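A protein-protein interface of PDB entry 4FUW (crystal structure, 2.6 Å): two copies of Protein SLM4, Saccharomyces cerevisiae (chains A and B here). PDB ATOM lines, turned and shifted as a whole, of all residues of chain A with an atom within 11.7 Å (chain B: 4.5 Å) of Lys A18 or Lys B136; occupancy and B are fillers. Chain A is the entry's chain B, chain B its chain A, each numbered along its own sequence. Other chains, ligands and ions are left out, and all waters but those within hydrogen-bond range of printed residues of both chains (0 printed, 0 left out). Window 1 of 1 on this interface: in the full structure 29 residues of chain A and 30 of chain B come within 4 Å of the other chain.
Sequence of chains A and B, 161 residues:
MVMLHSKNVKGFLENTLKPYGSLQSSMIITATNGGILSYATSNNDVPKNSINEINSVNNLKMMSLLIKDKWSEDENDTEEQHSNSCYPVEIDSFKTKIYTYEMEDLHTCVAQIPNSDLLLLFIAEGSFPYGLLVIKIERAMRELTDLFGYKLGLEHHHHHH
The backbone NH (N) of Leu B23 sits at hydrogen-bond distance from the backbone carbonyl oxygen (O) of Leu A17.
O of Thr A16 is in hydrogen-bond range of NZ of Lys B136 (2.7 Å).
Leu A132 touches Ile B135, and with the chains exchanged Ile A135 touches Leu B132.
Of the 13 pairs that touch across the chains among the printed residues, 2 have their exchanged pair printed and touching as well.
Of the 25 printed residues of chain A, 9 touch a printed residue of chain B.
Printed residues of chain A that touch a printed residue of chain B: Phe A12, Thr A16, Leu A17, Lys A18, Tyr A20, Pro A129, Gly A131, Leu A132 and Ile A135.
Hydrophobic or aromatic side chains of chain A within 4 Å of the printed part of chain B: Phe A12, Leu A17, Tyr A20, Pro A129 and Ile A135.
Of the 12 printed residues of chain B, 6 touch a printed residue of chain A.
Hydrophobic or aromatic side chains of chain B within 4 Å of the printed part of chain A: Leu B23, Phe B122, Leu B132, Ile B135 and Ala B140.
The side-chain hydroxyl of Thr A16 is in hydrogen-bond range of the backbone carbonyl oxygen of Leu A13 (2.5 Å).
OG of Ser A6 sits at hydrogen-bond distance from N of Phe A12 (2.8 Å).
OD1 of Asn A15 lies within hydrogen-bond range of NZ of Lys A18 (2.9 Å).
Of chain B, only Lys B136 comes within 4 Å of Lys A18.
Leu B132 touches just these residues of chain A: Tyr A20 and Ile A135.
No residue of chain A comes within 4 Å of Leu B133.
No residue of chain A comes within 4 Å of Val B134.
Ile B135 touches three residues of chain A.
Ile B137 touches none of the printed residues of chain A.
Ala B140 touches just these residues of chain A: Phe A12 (3.4 Å) and Thr A16 (3.8 Å).
Of the printed residues of chain B, Thr A16 touches Leu B23 (3.3 Å), Phe B122 (3.8 Å), Lys B136 (2.7 Å) and Ala B140 (3.8 Å).
Printed residues of chain B within 4 Å of Ile A135: Leu B132.
Lys A10 touches none of the printed residues of chain B.
Tyr A130 touches none of the printed residues of chain B.
The nearest printed residue of chain B that does not touch Leu A132 is Leu B132 (4.1 Å).
CZ of Phe A12 touches O of Ala B140 (3.4 Å).
Phe B122 touches Thr A16.
Thr A16 touches Ala B140 (CG2 to CB, 3.8 Å).
Lys A18 touches Lys B136 (O to NZ, 3.7 Å).
Leu B132 touches Tyr A20 (CD1 to CD2, 3.9 Å).
CG of Lys B136 touches CE2 of Tyr A20, at 3.8 Å.
Pro A129 touches Ile B135.
CD1 of Ile B135 touches C of Gly A131 (3.8 Å).
Ile B135 touches Leu A132.
Ile A135 touches Leu B132.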
ATOM      1  N   SER A   6      23.547 -14.195  -0.941  1.00  0.00           N
ATOM      2  CA  SER A   6      24.192 -13.299   0.066  1.00  0.00           C
ATOM      3  C   SER A   6      23.315 -13.089   1.296  1.00  0.00           C
ATOM      4  O   SER A   6      22.084 -13.169   1.206  1.00  0.00           O
ATOM      5  CB  SER A   6      24.495 -11.943  -0.560  1.00  0.00           C
ATOM      6  OG  SER A   6      24.862 -11.004   0.438  1.00  0.00           O
ATOM      7  N   LYS A   7      23.952 -12.795   2.437  1.00  0.00           N
ATOM      8  CA  LYS A   7      23.220 -12.557   3.696  1.00  0.00           C
ATOM      9  C   LYS A   7      23.129 -11.072   4.129  1.00  0.00           C
ATOM     10  O   LYS A   7      22.447 -10.753   5.113  1.00  0.00           O
ATOM     11  CB  LYS A   7      23.770 -13.435   4.842  1.00  0.00           C
ATOM     12  CG  LYS A   7      25.169 -13.059   5.318  1.00  0.00           C
ATOM     13  CD  LYS A   7      25.412 -13.436   6.777  1.00  0.00           C
ATOM     14  CE  LYS A   7      26.406 -12.485   7.435  1.00  0.00           C
ATOM     15  NZ  LYS A   7      27.591 -12.180   6.574  1.00  0.00           N
ATOM     16  N   ASN A   8      23.808 -10.177   3.404  1.00  0.00           N
ATOM     17  CA  ASN A   8      23.777  -8.734   3.699  1.00  0.00           C
ATOM     18  C   ASN A   8      24.220  -7.864   2.510  1.00  0.00           C
ATOM     19  O   ASN A   8      24.712  -8.386   1.506  1.00  0.00           O
ATOM     20  CB  ASN A   8      24.589  -8.408   4.966  1.00  0.00           C
ATOM     21  CG  ASN A   8      26.053  -8.767   4.838  1.00  0.00           C
ATOM     22  OD1 ASN A   8      26.927  -7.921   5.031  1.00  0.00           O
ATOM     23  ND2 ASN A   8      26.330 -10.029   4.523  1.00  0.00           N
ATOM     24  N   VAL A   9      24.051  -6.549   2.633  1.00  0.00           N
ATOM     25  CA  VAL A   9      24.248  -5.616   1.524  1.00  0.00           C
ATOM     26  C   VAL A   9      25.669  -5.645   0.929  1.00  0.00           C
ATOM     27  O   VAL A   9      25.825  -5.814  -0.285  1.00  0.00           O
ATOM     28  CB  VAL A   9      23.834  -4.183   1.919  1.00  0.00           C
ATOM     29  CG1 VAL A   9      24.145  -3.189   0.808  1.00  0.00           C
ATOM     30  CG2 VAL A   9      22.349  -4.151   2.231  1.00  0.00           C
ATOM     31  N   LYS A  10      26.687  -5.488   1.776  1.00  0.00           N
ATOM     32  CA  LYS A  10      28.081  -5.635   1.358  1.00  0.00           C
ATOM     33  C   LYS A  10      28.278  -6.935   0.544  1.00  0.00           C
ATOM     34  O   LYS A  10      28.794  -6.904  -0.578  1.00  0.00           O
ATOM     35  CB  LYS A  10      28.998  -5.618   2.586  1.00  0.00           C
ATOM     36  CG  LYS A  10      30.491  -5.682   2.291  1.00  0.00           C
ATOM     37  CD  LYS A  10      31.102  -4.305   2.084  1.00  0.00           C
ATOM     38  CE  LYS A  10      32.558  -4.420   1.638  1.00  0.00           C
ATOM     39  NZ  LYS A  10      33.143  -3.085   1.269  1.00  0.00           N
ATOM     40  N   GLY A  11      27.842  -8.059   1.114  1.00  0.00           N
ATOM     41  CA  GLY A  11      27.950  -9.369   0.478  1.00  0.00           C
ATOM     42  C   GLY A  11      27.233  -9.415  -0.855  1.00  0.00           C
ATOM     43  O   GLY A  11      27.758  -9.982  -1.822  1.00  0.00           O
ATOM     44  N   PHE A  12      26.036  -8.816  -0.909  1.00  0.00           N
ATOM     45  CA  PHE A  12      25.287  -8.707  -2.161  1.00  0.00           C
ATOM     46  C   PHE A  12      26.140  -8.009  -3.241  1.00  0.00           C
ATOM     47  O   PHE A  12      26.260  -8.503  -4.361  1.00  0.00           O
ATOM     48  CB  PHE A  12      23.942  -7.995  -1.949  1.00  0.00           C
ATOM     49  CG  PHE A  12      23.308  -7.516  -3.225  1.00  0.00           C
ATOM     50  CD1 PHE A  12      22.580  -8.384  -4.025  1.00  0.00           C
ATOM     51  CD2 PHE A  12      23.457  -6.192  -3.644  1.00  0.00           C
ATOM     52  CE1 PHE A  12      22.006  -7.948  -5.217  1.00  0.00           C
ATOM     53  CE2 PHE A  12      22.885  -5.748  -4.838  1.00  0.00           C
ATOM     54  CZ  PHE A  12      22.164  -6.631  -5.625  1.00  0.00           C
ATOM     55  N   LEU A  13      26.748  -6.884  -2.874  1.00  0.00           N
ATOM     56  CA  LEU A  13      27.527  -6.080  -3.792  1.00  0.00           C
ATOM     57  C   LEU A  13      28.814  -6.800  -4.224  1.00  0.00           C
ATOM     58  O   LEU A  13      29.176  -6.780  -5.396  1.00  0.00           O
ATOM     59  CB  LEU A  13      27.834  -4.709  -3.166  1.00  0.00           C
ATOM     60  CG  LEU A  13      26.628  -3.786  -2.953  1.00  0.00           C
ATOM     61  CD1 LEU A  13      27.055  -2.528  -2.225  1.00  0.00           C
ATOM     62  CD2 LEU A  13      25.929  -3.433  -4.261  1.00  0.00           C
ATOM     63  N   GLU A  14      29.492  -7.435  -3.266  1.00  0.00           N
ATOM     64  CA  GLU A  14      30.657  -8.282  -3.545  1.00  0.00           C
ATOM     65  C   GLU A  14      30.335  -9.369  -4.595  1.00  0.00           C
ATOM     66  O   GLU A  14      31.137  -9.636  -5.504  1.00  0.00           O
ATOM     67  CB  GLU A  14      31.199  -8.900  -2.246  1.00  0.00           C
ATOM     68  CG  GLU A  14      32.298  -8.057  -1.600  1.00  0.00           C
ATOM     69  CD  GLU A  14      32.597  -8.437  -0.144  1.00  0.00           C
ATOM     70  OE1 GLU A  14      33.149  -7.566   0.583  1.00  0.00           O
ATOM     71  OE2 GLU A  14      32.288  -9.592   0.284  1.00  0.00           O
ATOM     72  N   ASN A  15      29.147  -9.953  -4.473  1.00  0.00           N
ATOM     73  CA  ASN A  15      28.665 -10.918  -5.445  1.00  0.00           C
ATOM     74  C   ASN A  15      28.400 -10.327  -6.819  1.00  0.00           C
ATOM     75  O   ASN A  15      28.668 -10.989  -7.819  1.00  0.00           O
ATOM     76  CB  ASN A  15      27.439 -11.661  -4.917  1.00  0.00           C
ATOM     77  CG  ASN A  15      27.792 -12.586  -3.767  1.00  0.00           C
ATOM     78  OD1 ASN A  15      28.918 -13.087  -3.678  1.00  0.00           O
ATOM     79  ND2 ASN A  15      26.844 -12.806  -2.875  1.00  0.00           N
ATOM     80  N   THR A  16      27.908  -9.090  -6.870  1.00  0.00           N
ATOM     81  CA  THR A  16      27.701  -8.421  -8.158  1.00  0.00           C
ATOM     82  C   THR A  16      29.016  -8.173  -8.895  1.00  0.00           C
ATOM     83  O   THR A  16      29.017  -8.025 -10.106  1.00  0.00           O
ATOM     84  CB  THR A  16      26.923  -7.092  -8.050  1.00  0.00           C
ATOM     85  OG1 THR A  16      27.654  -6.164  -7.240  1.00  0.00           O
ATOM     86  CG2 THR A  16      25.499  -7.321  -7.485  1.00  0.00           C
ATOM     87  N   LEU A  17      30.131  -8.159  -8.171  1.00  0.00           N
ATOM     88  CA  LEU A  17      31.443  -7.970  -8.789  1.00  0.00           C
ATOM     89  C   LEU A  17      31.883  -9.193  -9.590  1.00  0.00           C
ATOM     90  O   LEU A  17      32.549  -9.062 -10.625  1.00  0.00           O
ATOM     91  CB  LEU A  17      32.503  -7.653  -7.726  1.00  0.00           C
ATOM     92  CG  LEU A  17      32.303  -6.431  -6.808  1.00  0.00           C
ATOM     93  CD1 LEU A  17      33.364  -6.406  -5.714  1.00  0.00           C
ATOM     94  CD2 LEU A  17      32.322  -5.130  -7.595  1.00  0.00           C
ATOM     95  N   LYS A  18      31.497 -10.373  -9.107  1.00  0.00           N
ATOM     96  CA  LYS A  18      32.002 -11.645  -9.608  1.00  0.00           C
ATOM     97  C   LYS A  18      31.639 -11.899 -11.067  1.00  0.00           C
ATOM     98  O   LYS A  18      30.514 -11.628 -11.482  1.00  0.00           O
ATOM     99  CB  LYS A  18      31.489 -12.785  -8.731  1.00  0.00           C
ATOM    100  CG  LYS A  18      32.214 -12.905  -7.397  1.00  0.00           C
ATOM    101  CD  LYS A  18      31.598 -14.039  -6.601  1.00  0.00           C
ATOM    102  CE  LYS A  18      32.016 -14.008  -5.146  1.00  0.00           C
ATOM    103  NZ  LYS A  18      31.043 -14.860  -4.398  1.00  0.00           N
ATOM    104  N   PRO A  19      32.597 -12.419 -11.851  1.00  0.00           N
ATOM    105  CA  PRO A  19      32.307 -12.800 -13.236  1.00  0.00           C
ATOM    106  C   PRO A  19      31.204 -13.857 -13.324  1.00  0.00           C
ATOM    107  O   PRO A  19      31.018 -14.642 -12.382  1.00  0.00           O
ATOM    108  CB  PRO A  19      33.632 -13.414 -13.710  1.00  0.00           C
ATOM    109  CG  PRO A  19      34.405 -13.744 -12.474  1.00  0.00           C
ATOM    110  CD  PRO A  19      34.001 -12.702 -11.480  1.00  0.00           C
ATOM    111  N   TYR A  20      30.465 -13.862 -14.435  1.00  0.00           N
ATOM    112  CA  TYR A  20      29.638 -15.020 -14.791  1.00  0.00           C
ATOM    113  C   TYR A  20      30.568 -16.201 -15.118  1.00  0.00           C
ATOM    114  O   TYR A  20      31.657 -15.996 -15.658  1.00  0.00           O
ATOM    115  CB  TYR A  20      28.739 -14.711 -15.988  1.00  0.00           C
ATOM    116  CG  TYR A  20      27.395 -14.120 -15.619  1.00  0.00           C
ATOM    117  CD1 TYR A  20      26.449 -14.872 -14.905  1.00  0.00           C
ATOM    118  CD2 TYR A  20      27.056 -12.821 -15.998  1.00  0.00           C
ATOM    119  CE1 TYR A  20      25.209 -14.338 -14.564  1.00  0.00           C
ATOM    120  CE2 TYR A  20      25.818 -12.273 -15.669  1.00  0.00           C
ATOM    121  CZ  TYR A  20      24.893 -13.031 -14.950  1.00  0.00           C
ATOM    122  OH  TYR A  20      23.658 -12.492 -14.611  1.00  0.00           O
ATOM    123  N   GLY A  21      30.155 -17.424 -14.786  1.00  0.00           N
ATOM    124  CA  GLY A  21      30.970 -18.614 -15.053  1.00  0.00           C
ATOM    125  C   GLY A  21      31.279 -18.945 -16.523  1.00  0.00           C
ATOM    126  O   GLY A  21      30.829 -18.265 -17.467  1.00  0.00           O
ATOM    127  N   SER A  22      32.058 -20.008 -16.700  1.00  0.00           N
ATOM    128  CA  SER A  22      32.448 -20.508 -18.015  1.00  0.00           C
ATOM    129  C   SER A  22      31.252 -20.902 -18.888  1.00  0.00           C
ATOM    130  O   SER A  22      30.142 -21.141 -18.387  1.00  0.00           O
ATOM    131  CB  SER A  22      33.380 -21.723 -17.864  1.00  0.00           C
ATOM    132  OG  SER A  22      34.623 -21.370 -17.285  1.00  0.00           O
ATOM    133  N   SER A 127      21.344 -21.177 -16.360  1.00  0.00           N
ATOM    134  CA  SER A 127      21.415 -19.933 -15.627  1.00  0.00           C
ATOM    135  C   SER A 127      22.135 -18.828 -16.411  1.00  0.00           C
ATOM    136  O   SER A 127      21.951 -17.645 -16.129  1.00  0.00           O
ATOM    137  CB  SER A 127      22.147 -20.186 -14.315  1.00  0.00           C
ATOM    138  OG  SER A 127      23.407 -20.778 -14.569  1.00  0.00           O
ATOM    139  N   PHE A 128      22.969 -19.218 -17.375  1.00  0.00           N
ATOM    140  CA  PHE A 128      23.703 -18.286 -18.242  1.00  0.00           C
ATOM    141  C   PHE A 128      22.703 -17.535 -19.115  1.00  0.00           C
ATOM    142  O   PHE A 128      21.934 -18.161 -19.838  1.00  0.00           O
ATOM    143  CB  PHE A 128      24.656 -19.089 -19.123  1.00  0.00           C
ATOM    144  CG  PHE A 128      25.866 -18.332 -19.603  1.00  0.00           C
ATOM    145  CD1 PHE A 128      25.791 -17.499 -20.711  1.00  0.00           C
ATOM    146  CD2 PHE A 128      27.098 -18.511 -18.980  1.00  0.00           C
ATOM    147  CE1 PHE A 128      26.917 -16.824 -21.167  1.00  0.00           C
ATOM    148  CE2 PHE A 128      28.235 -17.834 -19.428  1.00  0.00           C
ATOM    149  CZ  PHE A 128      28.142 -16.984 -20.528  1.00  0.00           C
ATOM    150  N   PRO A 129      22.698 -16.192 -19.051  1.00  0.00           N
ATOM    151  CA  PRO A 129      21.669 -15.447 -19.774  1.00  0.00           C
ATOM    152  C   PRO A 129      21.868 -15.475 -21.293  1.00  0.00           C
ATOM    153  O   PRO A 129      22.988 -15.261 -21.789  1.00  0.00           O
ATOM    154  CB  PRO A 129      21.816 -14.010 -19.236  1.00  0.00           C
ATOM    155  CG  PRO A 129      22.862 -14.051 -18.158  1.00  0.00           C
ATOM    156  CD  PRO A 129      23.654 -15.300 -18.371  1.00  0.00           C
ATOM    157  N   TYR A 130      20.780 -15.729 -22.018  1.00  0.00           N
ATOM    158  CA  TYR A 130      20.802 -15.744 -23.475  1.00  0.00           C
ATOM    159  C   TYR A 130      21.465 -14.512 -24.048  1.00  0.00           C
ATOM    160  O   TYR A 130      22.273 -14.620 -24.980  1.00  0.00           O
ATOM    161  CB  TYR A 130      19.396 -15.870 -24.045  1.00  0.00           C
ATOM    162  CG  TYR A 130      18.812 -17.266 -23.978  1.00  0.00           C
ATOM    163  CD1 TYR A 130      19.419 -18.345 -24.648  1.00  0.00           C
ATOM    164  CD2 TYR A 130      17.634 -17.512 -23.260  1.00  0.00           C
ATOM    165  CE1 TYR A 130      18.871 -19.621 -24.589  1.00  0.00           C
ATOM    166  CE2 TYR A 130      17.083 -18.780 -23.197  1.00  0.00           C
ATOM    167  CZ  TYR A 130      17.697 -19.831 -23.865  1.00  0.00           C
ATOM    168  OH  TYR A 130      17.133 -21.085 -23.785  1.00  0.00           O
ATOM    169  N   GLY A 131      21.132 -13.348 -23.489  1.00  0.00           N
ATOM    170  CA  GLY A 131      21.681 -12.075 -23.960  1.00  0.00           C
ATOM    171  C   GLY A 131      23.199 -12.030 -23.953  1.00  0.00           C
ATOM    172  O   GLY A 131      23.811 -11.463 -24.865  1.00  0.00           O
ATOM    173  N   LEU A 132      23.815 -12.634 -22.933  1.00  0.00           N
ATOM    174  CA  LEU A 132      25.275 -12.674 -22.832  1.00  0.00           C
ATOM    175  C   LEU A 132      25.884 -13.594 -23.891  1.00  0.00           C
ATOM    176  O   LEU A 132      26.975 -13.318 -24.412  1.00  0.00           O
ATOM    177  CB  LEU A 132      25.718 -13.084 -21.425  1.00  0.00           C
ATOM    178  CG  LEU A 132      27.209 -13.363 -21.140  1.00  0.00           C
ATOM    179  CD1 LEU A 132      28.157 -12.241 -21.563  1.00  0.00           C
ATOM    180  CD2 LEU A 132      27.427 -13.697 -19.668  1.00  0.00           C
ATOM    181  N   LEU A 133      25.187 -14.681 -24.214  1.00  0.00           N
ATOM    182  CA  LEU A 133      25.632 -15.547 -25.296  1.00  0.00           C
ATOM    183  C   LEU A 133      25.693 -14.781 -26.618  1.00  0.00           C
ATOM    184  O   LEU A 133      26.701 -14.851 -27.329  1.00  0.00           O
ATOM    185  CB  LEU A 133      24.754 -16.793 -25.410  1.00  0.00           C
ATOM    186  CG  LEU A 133      24.953 -17.796 -24.275  1.00  0.00           C
ATOM    187  CD1 LEU A 133      23.859 -18.833 -24.308  1.00  0.00           C
ATOM    188  CD2 LEU A 133      26.313 -18.460 -24.339  1.00  0.00           C
ATOM    189  N   ILE A 135      26.089 -11.549 -27.082  1.00  0.00           N
ATOM    190  CA  ILE A 135      27.202 -10.616 -27.022  1.00  0.00           C
ATOM    191  C   ILE A 135      28.526 -11.341 -27.271  1.00  0.00           C
ATOM    192  O   ILE A 135      29.316 -10.919 -28.117  1.00  0.00           O
ATOM    193  CB  ILE A 135      27.187  -9.828 -25.680  1.00  0.00           C
ATOM    194  CG1 ILE A 135      25.979  -8.880 -25.666  1.00  0.00           C
ATOM    195  CG2 ILE A 135      28.481  -9.054 -25.467  1.00  0.00           C
ATOM    196  CD1 ILE A 135      25.547  -8.405 -24.297  1.00  0.00           C
ATOM    197  N   LEU B  23      33.599  -6.659 -12.041  1.00  0.00           N
ATOM    198  CA  LEU B  23      33.351  -5.235 -12.081  1.00  0.00           C
ATOM    199  C   LEU B  23      34.542  -4.573 -11.395  1.00  0.00           C
ATOM    200  O   LEU B  23      35.246  -5.200 -10.602  1.00  0.00           O
ATOM    201  CB  LEU B  23      32.052  -4.897 -11.351  1.00  0.00           C
ATOM    202  CG  LEU B  23      30.719  -5.336 -11.972  1.00  0.00           C
ATOM    203  CD1 LEU B  23      29.574  -4.910 -11.067  1.00  0.00           C
ATOM    204  CD2 LEU B  23      30.537  -4.771 -13.375  1.00  0.00           C
ATOM    205  N   PHE B 122      27.005   0.190 -11.121  1.00  0.00           N
ATOM    206  CA  PHE B 122      28.129  -0.679 -11.473  1.00  0.00           C
ATOM    207  C   PHE B 122      29.146   0.119 -12.267  1.00  0.00           C
ATOM    208  O   PHE B 122      28.781   0.887 -13.174  1.00  0.00           O
ATOM    209  CB  PHE B 122      27.686  -1.874 -12.324  1.00  0.00           C
ATOM    210  CG  PHE B 122      26.770  -2.842 -11.623  1.00  0.00           C
ATOM    211  CD1 PHE B 122      26.606  -2.818 -10.243  1.00  0.00           C
ATOM    212  CD2 PHE B 122      26.094  -3.815 -12.361  1.00  0.00           C
ATOM    213  CE1 PHE B 122      25.760  -3.724  -9.618  1.00  0.00           C
ATOM    214  CE2 PHE B 122      25.250  -4.733 -11.743  1.00  0.00           C
ATOM    215  CZ  PHE B 122      25.078  -4.687 -10.365  1.00  0.00           C
ATOM    216  N   PHE B 128      34.455  -3.855 -20.919  1.00  0.00           N
ATOM    217  CA  PHE B 128      33.302  -4.586 -20.413  1.00  0.00           C
ATOM    218  C   PHE B 128      32.075  -4.154 -21.207  1.00  0.00           C
ATOM    219  O   PHE B 128      31.756  -2.968 -21.247  1.00  0.00           O
ATOM    220  CB  PHE B 128      33.128  -4.276 -18.931  1.00  0.00           C
ATOM    221  CG  PHE B 128      32.297  -5.272 -18.180  1.00  0.00           C
ATOM    222  CD1 PHE B 128      30.910  -5.262 -18.282  1.00  0.00           C
ATOM    223  CD2 PHE B 128      32.901  -6.187 -17.337  1.00  0.00           C
ATOM    224  CE1 PHE B 128      30.145  -6.169 -17.572  1.00  0.00           C
ATOM    225  CE2 PHE B 128      32.142  -7.104 -16.623  1.00  0.00           C
ATOM    226  CZ  PHE B 128      30.760  -7.092 -16.737  1.00  0.00           C
ATOM    227  N   LEU B 132      26.131  -6.292 -21.059  1.00  0.00           N
ATOM    228  CA  LEU B 132      26.296  -7.168 -19.909  1.00  0.00           C
ATOM    229  C   LEU B 132      26.022  -6.428 -18.604  1.00  0.00           C
ATOM    230  O   LEU B 132      25.437  -6.992 -17.673  1.00  0.00           O
ATOM    231  CB  LEU B 132      27.688  -7.795 -19.905  1.00  0.00           C
ATOM    232  CG  LEU B 132      28.128  -8.650 -18.711  1.00  0.00           C
ATOM    233  CD1 LEU B 132      27.113  -9.711 -18.302  1.00  0.00           C
ATOM    234  CD2 LEU B 132      29.474  -9.285 -19.027  1.00  0.00           C
ATOM    235  N   LEU B 133      26.441  -5.169 -18.536  1.00  0.00           N
ATOM    236  CA  LEU B 133      26.087  -4.327 -17.402  1.00  0.00           C
ATOM    237  C   LEU B 133      24.564  -4.262 -17.244  1.00  0.00           C
ATOM    238  O   LEU B 133      24.046  -4.530 -16.145  1.00  0.00           O
ATOM    239  CB  LEU B 133      26.702  -2.939 -17.541  1.00  0.00           C
ATOM    240  CG  LEU B 133      28.214  -2.887 -17.326  1.00  0.00           C
ATOM    241  CD1 LEU B 133      28.750  -1.510 -17.665  1.00  0.00           C
ATOM    242  CD2 LEU B 133      28.596  -3.266 -15.909  1.00  0.00           C
ATOM    243  N   VAL B 134      23.860  -3.959 -18.344  1.00  0.00           N
ATOM    244  CA  VAL B 134      22.389  -3.921 -18.373  1.00  0.00           C
ATOM    245  C   VAL B 134      21.766  -5.220 -17.864  1.00  0.00           C
ATOM    246  O   VAL B 134      20.848  -5.200 -17.028  1.00  0.00           O
ATOM    247  CB  VAL B 134      21.841  -3.600 -19.783  1.00  0.00           C
ATOM    248  CG1 VAL B 134      20.351  -3.905 -19.876  1.00  0.00           C
ATOM    249  CG2 VAL B 134      22.096  -2.141 -20.136  1.00  0.00           C
ATOM    250  N   ILE B 135      22.276  -6.342 -18.363  1.00  0.00           N
ATOM    251  CA  ILE B 135      21.824  -7.658 -17.923  1.00  0.00           C
ATOM    252  C   ILE B 135      22.084  -7.856 -16.422  1.00  0.00           C
ATOM    253  O   ILE B 135      21.156  -8.165 -15.671  1.00  0.00           O
ATOM    254  CB  ILE B 135      22.424  -8.788 -18.811  1.00  0.00           C
ATOM    255  CG1 ILE B 135      21.727  -8.783 -20.176  1.00  0.00           C
ATOM    256  CG2 ILE B 135      22.269 -10.159 -18.161  1.00  0.00           C
ATOM    257  CD1 ILE B 135      22.545  -9.364 -21.313  1.00  0.00           C
ATOM    258  N   LYS B 136      23.328  -7.660 -15.991  1.00  0.00           N
ATOM    259  CA  LYS B 136      23.698  -7.847 -14.590  1.00  0.00           C
ATOM    260  C   LYS B 136      22.875  -6.976 -13.646  1.00  0.00           C
ATOM    261  O   LYS B 136      22.384  -7.453 -12.630  1.00  0.00           O
ATOM    262  CB  LYS B 136      25.172  -7.536 -14.374  1.00  0.00           C
ATOM    263  CG  LYS B 136      26.121  -8.641 -14.758  1.00  0.00           C
ATOM    264  CD  LYS B 136      27.557  -8.204 -14.509  1.00  0.00           C
ATOM    265  CE  LYS B 136      27.813  -7.939 -13.038  1.00  0.00           C
ATOM    266  NZ  LYS B 136      27.816  -9.213 -12.273  1.00  0.00           N
ATOM    267  N   ILE B 137      22.725  -5.698 -13.984  1.00  0.00           N
ATOM    268  CA  ILE B 137      22.035  -4.779 -13.086  1.00  0.00           C
ATOM    269  C   ILE B 137      20.535  -5.116 -12.939  1.00  0.00           C
ATOM    270  O   ILE B 137      19.970  -4.956 -11.843  1.00  0.00           O
ATOM    271  CB  ILE B 137      22.327  -3.297 -13.417  1.00  0.00           C
ATOM    272  CG1 ILE B 137      22.153  -2.426 -12.182  1.00  0.00           C
ATOM    273  CG2 ILE B 137      21.461  -2.807 -14.560  1.00  0.00           C
ATOM    274  CD1 ILE B 137      23.115  -1.261 -12.114  1.00  0.00           C
ATOM    275  N   GLU B 138      19.910  -5.614 -14.012  1.00  0.00           N
ATOM    276  CA  GLU B 138      18.532  -6.095 -13.908  1.00  0.00           C
ATOM    277  C   GLU B 138      18.419  -7.350 -13.052  1.00  0.00           C
ATOM    278  O   GLU B 138      17.500  -7.471 -12.258  1.00  0.00           O
ATOM    279  CB  GLU B 138      17.873  -6.339 -15.259  1.00  0.00           C
ATOM    280  CG  GLU B 138      16.379  -6.574 -15.083  1.00  0.00           C
ATOM    281  CD  GLU B 138      15.687  -7.089 -16.317  1.00  0.00           C
ATOM    282  OE1 GLU B 138      16.234  -6.912 -17.429  1.00  0.00           O
ATOM    283  OE2 GLU B 138      14.581  -7.661 -16.164  1.00  0.00           O
ATOM    284  N   ARG B 139      19.346  -8.282 -13.219  1.00  0.00           N
ATOM    285  CA  ARG B 139      19.371  -9.476 -12.384  1.00  0.00           C
ATOM    286  C   ARG B 139      19.584  -9.086 -10.905  1.00  0.00           C
ATOM    287  O   ARG B 139      18.802  -9.482 -10.042  1.00  0.00           O
ATOM    288  CB  ARG B 139      20.435 -10.466 -12.898  1.00  0.00           C
ATOM    289  CG  ARG B 139      20.781 -11.613 -11.956  1.00  0.00           C
ATOM    290  CD  ARG B 139      19.787 -12.756 -12.079  1.00  0.00           C
ATOM    291  NE  ARG B 139      19.504 -13.369 -10.780  1.00  0.00           N
ATOM    292  CZ  ARG B 139      18.403 -13.149 -10.059  1.00  0.00           C
ATOM    293  NH1 ARG B 139      18.253 -13.757  -8.892  1.00  0.00           N
ATOM    294  NH2 ARG B 139      17.449 -12.332 -10.499  1.00  0.00           N
ATOM    295  N   ALA B 140      20.614  -8.283 -10.632  1.00  0.00           N
ATOM    296  CA  ALA B 140      20.914  -7.807  -9.272  1.00  0.00           C
ATOM    297  C   ALA B 140      19.739  -7.060  -8.646  1.00  0.00           C
ATOM    298  O   ALA B 140      19.399  -7.290  -7.479  1.00  0.00           O
ATOM    299  CB  ALA B 140      22.159  -6.940  -9.261  1.00  0.00           C
